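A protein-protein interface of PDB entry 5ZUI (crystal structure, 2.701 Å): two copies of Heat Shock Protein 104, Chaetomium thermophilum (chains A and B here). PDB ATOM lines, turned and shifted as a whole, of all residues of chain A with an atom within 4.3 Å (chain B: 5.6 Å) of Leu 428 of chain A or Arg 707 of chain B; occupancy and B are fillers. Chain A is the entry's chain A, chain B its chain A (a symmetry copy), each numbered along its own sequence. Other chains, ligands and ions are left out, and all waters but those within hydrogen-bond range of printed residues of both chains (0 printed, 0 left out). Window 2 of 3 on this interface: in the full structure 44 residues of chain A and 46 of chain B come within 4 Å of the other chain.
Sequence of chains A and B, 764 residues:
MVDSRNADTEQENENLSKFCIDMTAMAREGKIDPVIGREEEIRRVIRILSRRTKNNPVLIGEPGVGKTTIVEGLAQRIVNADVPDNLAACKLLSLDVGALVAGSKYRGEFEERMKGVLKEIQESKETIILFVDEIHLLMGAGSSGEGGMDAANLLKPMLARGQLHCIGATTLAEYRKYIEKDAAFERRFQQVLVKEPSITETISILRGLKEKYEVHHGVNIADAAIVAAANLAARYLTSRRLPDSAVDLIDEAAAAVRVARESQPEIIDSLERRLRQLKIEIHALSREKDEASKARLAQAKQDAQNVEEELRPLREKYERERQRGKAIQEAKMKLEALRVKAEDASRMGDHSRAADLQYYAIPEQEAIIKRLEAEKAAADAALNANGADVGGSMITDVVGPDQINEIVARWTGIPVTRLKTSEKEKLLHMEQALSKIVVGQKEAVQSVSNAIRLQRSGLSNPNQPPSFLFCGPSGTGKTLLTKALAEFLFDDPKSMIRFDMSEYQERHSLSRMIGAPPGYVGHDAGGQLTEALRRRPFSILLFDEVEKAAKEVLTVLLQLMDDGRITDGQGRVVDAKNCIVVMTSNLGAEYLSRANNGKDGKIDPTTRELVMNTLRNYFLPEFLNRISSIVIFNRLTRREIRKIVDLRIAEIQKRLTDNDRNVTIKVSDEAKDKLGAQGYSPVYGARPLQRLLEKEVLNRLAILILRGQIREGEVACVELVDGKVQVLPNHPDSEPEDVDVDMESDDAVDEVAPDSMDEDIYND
The backbone carbonyl oxygen (O) of Leu 427 of chain A is in hydrogen-bond range of the guanidinium group (NH1) of Arg 453 of chain A (2.6 Å).
Among the printed residues, pairs that only touch across the chains: Lys 424 of chain A with Leu 706 of chain B, Leu 427 of chain A with Leu 706 of chain B, Leu 428 of chain A with Ile 703 of chain B, Leu 428 of chain A with Arg 707 of chain B, Arg 453 of chain A with Ala 702 of chain B and Arg 453 of chain A with Ile 703 of chain B.
Of the 8 printed residues of chain A, 4 touch a printed residue of chain B. Printed residues of chain B that touch a printed residue of chain A: Ala 702, Ile 703, Leu 706 and Arg 707. Hydrophobic or aromatic side chains of chain B that line the printed part of chain A: Ala 702, Ile 703 and Leu 706.
No position is printed for both chains. Of the 6 pairs that touch across the chains among the printed residues, none has its exchanged pair printed and touching as well.
Leu 428 of chain A touches just these residues of chain B: Ile 703 and Arg 707. His 429 of chain A touches none of the printed residues of chain B. Printed residues of chain B within 4 Å of Arg 453 of chain A: Ala 702 and Ile 703. Of the printed residues of chain A, Ile 703 of chain B touches Leu 428 (3.7 Å) and Arg 453 (3.5 Å). Of the printed residues of chain A, Leu 706 of chain B touches Lys 424 (3.8 Å) and Leu 427 (3.7 Å). Printed residues of chain A within 4 Å of Arg 707 of chain B: Leu 428 (3.7 Å). The nearest printed residue of chain B that does not touch Leu 427 of chain A is Ile 703 of chain B (6.4 Å).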
ATOM      1  N   LYS A 424     -33.403  28.700 -28.479  1.00  0.00           N
ATOM      2  CA  LYS A 424     -32.518  27.569 -28.216  1.00  0.00           C
ATOM      3  C   LYS A 424     -32.705  26.452 -29.238  1.00  0.00           C
ATOM      4  O   LYS A 424     -31.746  25.742 -29.563  1.00  0.00           O
ATOM      5  CB  LYS A 424     -32.750  27.036 -26.797  1.00  0.00           C
ATOM      6  CG  LYS A 424     -33.213  28.087 -25.789  1.00  0.00           C
ATOM      7  CD  LYS A 424     -33.705  27.437 -24.495  1.00  0.00           C
ATOM      8  CE  LYS A 424     -34.520  28.409 -23.641  1.00  0.00           C
ATOM      9  NZ  LYS A 424     -33.666  29.387 -22.896  1.00  0.00           N
ATOM     10  N   GLU A 425     -33.920  26.277 -29.760  1.00  0.00           N
ATOM     11  CA  GLU A 425     -34.144  25.216 -30.736  1.00  0.00           C
ATOM     12  C   GLU A 425     -33.468  25.541 -32.062  1.00  0.00           C
ATOM     13  O   GLU A 425     -32.764  24.699 -32.631  1.00  0.00           O
ATOM     14  CB  GLU A 425     -35.643  24.975 -30.928  1.00  0.00           C
ATOM     15  CG  GLU A 425     -36.047  23.509 -30.772  1.00  0.00           C
ATOM     16  CD  GLU A 425     -37.536  23.277 -30.970  1.00  0.00           C
ATOM     17  OE1 GLU A 425     -38.002  23.344 -32.129  1.00  0.00           O
ATOM     18  OE2 GLU A 425     -38.240  23.023 -29.966  1.00  0.00           O
ATOM     19  N   LYS A 426     -33.670  26.761 -32.568  1.00  0.00           N
ATOM     20  CA  LYS A 426     -33.026  27.169 -33.814  1.00  0.00           C
ATOM     21  C   LYS A 426     -31.514  27.020 -33.721  1.00  0.00           C
ATOM     22  O   LYS A 426     -30.875  26.443 -34.610  1.00  0.00           O
ATOM     23  CB  LYS A 426     -33.388  28.619 -34.146  1.00  0.00           C
ATOM     24  CG  LYS A 426     -34.865  28.968 -34.074  1.00  0.00           C
ATOM     25  CD  LYS A 426     -35.125  30.368 -34.636  1.00  0.00           C
ATOM     26  CE  LYS A 426     -34.043  31.357 -34.205  1.00  0.00           C
ATOM     27  NZ  LYS A 426     -34.356  32.765 -34.599  1.00  0.00           N
ATOM     28  N   LEU A 427     -30.926  27.529 -32.638  1.00  0.00           N
ATOM     29  CA  LEU A 427     -29.474  27.571 -32.522  1.00  0.00           C
ATOM     30  C   LEU A 427     -28.861  26.175 -32.472  1.00  0.00           C
ATOM     31  O   LEU A 427     -27.717  25.986 -32.904  1.00  0.00           O
ATOM     32  CB  LEU A 427     -29.080  28.372 -31.280  1.00  0.00           C
ATOM     33  CG  LEU A 427     -28.980  29.897 -31.386  1.00  0.00           C
ATOM     34  CD1 LEU A 427     -30.027  30.492 -32.316  1.00  0.00           C
ATOM     35  CD2 LEU A 427     -29.094  30.514 -30.004  1.00  0.00           C
ATOM     36  N   LEU A 428     -29.600  25.191 -31.953  1.00  0.00           N
ATOM     37  CA  LEU A 428     -29.060  23.838 -31.864  1.00  0.00           C
ATOM     38  C   LEU A 428     -28.973  23.171 -33.232  1.00  0.00           C
ATOM     39  O   LEU A 428     -28.080  22.347 -33.459  1.00  0.00           O
ATOM     40  CB  LEU A 428     -29.905  22.997 -30.910  1.00  0.00           C
ATOM     41  CG  LEU A 428     -29.632  23.221 -29.420  1.00  0.00           C
ATOM     42  CD1 LEU A 428     -30.742  22.618 -28.575  1.00  0.00           C
ATOM     43  CD2 LEU A 428     -28.273  22.660 -29.009  1.00  0.00           C
ATOM     44  N   HIS A 429     -29.878  23.514 -34.153  1.00  0.00           N
ATOM     45  CA  HIS A 429     -29.842  23.018 -35.525  1.00  0.00           C
ATOM     46  C   HIS A 429     -29.473  24.120 -36.513  1.00  0.00           C
ATOM     47  O   HIS A 429     -29.957  24.137 -37.649  1.00  0.00           O
ATOM     48  CB  HIS A 429     -31.180  22.390 -35.904  1.00  0.00           C
ATOM     49  CG  HIS A 429     -31.714  21.447 -34.872  1.00  0.00           C
ATOM     50  ND1 HIS A 429     -32.707  21.800 -33.985  1.00  0.00           N
ATOM     51  CD2 HIS A 429     -31.385  20.167 -34.580  1.00  0.00           C
ATOM     52  CE1 HIS A 429     -32.970  20.778 -33.192  1.00  0.00           C
ATOM     53  NE2 HIS A 429     -32.181  19.775 -33.531  1.00  0.00           N
ATOM     54  N   MET A 430     -28.616  25.051 -36.087  1.00  0.00           N
ATOM     55  CA  MET A 430     -28.264  26.182 -36.936  1.00  0.00           C
ATOM     56  C   MET A 430     -27.524  25.728 -38.188  1.00  0.00           C
ATOM     57  O   MET A 430     -27.779  26.236 -39.290  1.00  0.00           O
ATOM     58  CB  MET A 430     -27.420  27.179 -36.145  1.00  0.00           C
ATOM     59  CG  MET A 430     -27.205  28.495 -36.857  1.00  0.00           C
ATOM     60  SD  MET A 430     -26.248  29.663 -35.886  1.00  0.00           S
ATOM     61  CE  MET A 430     -26.919  31.201 -36.494  1.00  0.00           C
ATOM     62  N   ARG A 453     -23.756  30.493 -30.929  1.00  0.00           N
ATOM     63  CA  ARG A 453     -24.105  29.695 -29.759  1.00  0.00           C
ATOM     64  C   ARG A 453     -23.287  30.103 -28.542  1.00  0.00           C
ATOM     65  O   ARG A 453     -23.774  30.023 -27.411  1.00  0.00           O
ATOM     66  CB  ARG A 453     -23.915  28.206 -30.054  1.00  0.00           C
ATOM     67  CG  ARG A 453     -25.103  27.557 -30.745  1.00  0.00           C
ATOM     68  CD  ARG A 453     -25.013  26.054 -30.685  1.00  0.00           C
ATOM     69  NE  ARG A 453     -23.942  25.530 -31.522  1.00  0.00           N
ATOM     70  CZ  ARG A 453     -24.118  25.124 -32.774  1.00  0.00           C
ATOM     71  NH1 ARG A 453     -25.320  25.190 -33.333  1.00  0.00           N
ATOM     72  NH2 ARG A 453     -23.093  24.653 -33.469  1.00  0.00           N
ATOM     73  N   ALA B 702     -21.276  25.295 -24.692  1.00  0.00           N
ATOM     74  CA  ALA B 702     -22.418  26.050 -25.193  1.00  0.00           C
ATOM     75  C   ALA B 702     -23.590  25.121 -25.500  1.00  0.00           C
ATOM     76  O   ALA B 702     -24.639  25.192 -24.852  1.00  0.00           O
ATOM     77  CB  ALA B 702     -22.013  26.847 -26.429  1.00  0.00           C
ATOM     78  N   ILE B 703     -23.401  24.211 -26.463  1.00  0.00           N
ATOM     79  CA  ILE B 703     -24.476  23.332 -26.928  1.00  0.00           C
ATOM     80  C   ILE B 703     -25.187  22.658 -25.755  1.00  0.00           C
ATOM     81  O   ILE B 703     -26.422  22.625 -25.687  1.00  0.00           O
ATOM     82  CB  ILE B 703     -23.918  22.291 -27.916  1.00  0.00           C
ATOM     83  CG1 ILE B 703     -23.465  22.978 -29.209  1.00  0.00           C
ATOM     84  CG2 ILE B 703     -24.959  21.226 -28.205  1.00  0.00           C
ATOM     85  CD1 ILE B 703     -22.599  22.121 -30.091  1.00  0.00           C
ATOM     86  N   LEU B 704     -24.417  22.112 -24.807  1.00  0.00           N
ATOM     87  CA  LEU B 704     -25.040  21.425 -23.677  1.00  0.00           C
ATOM     88  C   LEU B 704     -25.861  22.366 -22.811  1.00  0.00           C
ATOM     89  O   LEU B 704     -26.884  21.954 -22.252  1.00  0.00           O
ATOM     90  CB  LEU B 704     -23.980  20.703 -22.838  1.00  0.00           C
ATOM     91  CG  LEU B 704     -23.288  19.608 -23.645  1.00  0.00           C
ATOM     92  CD1 LEU B 704     -22.043  19.099 -22.927  1.00  0.00           C
ATOM     93  CD2 LEU B 704     -24.271  18.465 -23.998  1.00  0.00           C
ATOM     94  N   ILE B 705     -25.426  23.616 -22.665  1.00  0.00           N
ATOM     95  CA  ILE B 705     -26.206  24.583 -21.898  1.00  0.00           C
ATOM     96  C   ILE B 705     -27.549  24.853 -22.575  1.00  0.00           C
ATOM     97  O   ILE B 705     -28.609  24.767 -21.943  1.00  0.00           O
ATOM     98  CB  ILE B 705     -25.400  25.878 -21.696  1.00  0.00           C
ATOM     99  CG1 ILE B 705     -24.359  25.687 -20.588  1.00  0.00           C
ATOM    100  CG2 ILE B 705     -26.302  27.050 -21.354  1.00  0.00           C
ATOM    101  CD1 ILE B 705     -23.416  26.849 -20.451  1.00  0.00           C
ATOM    102  N   LEU B 706     -27.530  25.172 -23.872  1.00  0.00           N
ATOM    103  CA  LEU B 706     -28.789  25.461 -24.550  1.00  0.00           C
ATOM    104  C   LEU B 706     -29.642  24.219 -24.741  1.00  0.00           C
ATOM    105  O   LEU B 706     -30.861  24.346 -24.905  1.00  0.00           O
ATOM    106  CB  LEU B 706     -28.564  26.128 -25.908  1.00  0.00           C
ATOM    107  CG  LEU B 706     -27.716  27.394 -26.037  1.00  0.00           C
ATOM    108  CD1 LEU B 706     -26.275  27.048 -26.299  1.00  0.00           C
ATOM    109  CD2 LEU B 706     -28.282  28.266 -27.153  1.00  0.00           C
ATOM    110  N   ARG B 707     -29.038  23.025 -24.724  1.00  0.00           N
ATOM    111  CA  ARG B 707     -29.808  21.785 -24.775  1.00  0.00           C
ATOM    112  C   ARG B 707     -30.458  21.449 -23.439  1.00  0.00           C
ATOM    113  O   ARG B 707     -31.356  20.601 -23.394  1.00  0.00           O
ATOM    114  CB  ARG B 707     -28.910  20.619 -25.201  1.00  0.00           C
ATOM    115  CG  ARG B 707     -29.295  19.942 -26.508  1.00  0.00           C
ATOM    116  CD  ARG B 707     -28.282  18.854 -26.854  1.00  0.00           C
ATOM    117  NE  ARG B 707     -27.853  18.903 -28.250  1.00  0.00           N
ATOM    118  CZ  ARG B 707     -26.804  18.243 -28.733  1.00  0.00           C
ATOM    119  NH1 ARG B 707     -26.065  17.487 -27.927  1.00  0.00           N
ATOM    120  NH2 ARG B 707     -26.489  18.341 -30.021  1.00  0.00           N
ATOM    121  N   GLY B 708     -30.027  22.091 -22.357  1.00  0.00           N
ATOM    122  CA  GLY B 708     -30.502  21.749 -21.036  1.00  0.00           C
ATOM    123  C   GLY B 708     -29.844  20.538 -20.418  1.00  0.00           C
ATOM    124  O   GLY B 708     -30.336  20.038 -19.402  1.00  0.00           O
ATOM    125  N   GLN B 709     -28.754  20.041 -21.001  1.00  0.00           N
ATOM    126  CA  GLN B 709     -28.033  18.922 -20.413  1.00  0.00           C
ATOM    127  C   GLN B 709     -27.073  19.354 -19.314  1.00  0.00           C
ATOM    128  O   GLN B 709     -26.531  18.488 -18.618  1.00  0.00           O
ATOM    129  CB  GLN B 709     -27.280  18.158 -21.502  1.00  0.00           C
ATOM    130  CG  GLN B 709     -28.098  17.936 -22.767  1.00  0.00           C
ATOM    131  CD  GLN B 709     -27.592  16.771 -23.589  1.00  0.00           C
ATOM    132  OE1 GLN B 709     -26.587  16.145 -23.251  1.00  0.00           O
ATOM    133  NE2 GLN B 709     -28.286  16.473 -24.680  1.00  0.00           N
ATOM    134  N   ASP B 733     -30.358  13.752 -23.278  1.00  0.00           N
ATOM    135  CA  ASP B 733     -31.235  14.574 -24.107  1.00  0.00           C
ATOM    136  C   ASP B 733     -32.714  14.284 -23.859  1.00  0.00           C
ATOM    137  O   ASP B 733     -33.472  15.165 -23.448  1.00  0.00           O
ATOM    138  CB  ASP B 733     -30.897  14.358 -25.588  1.00  0.00           C
ATOM    139  CG  ASP B 733     -31.637  15.313 -26.507  1.00  0.00           C
ATOM    140  OD1 ASP B 733     -32.844  15.089 -26.751  1.00  0.00           O
ATOM    141  OD2 ASP B 733     -31.007  16.281 -26.991  1.00  0.00           O
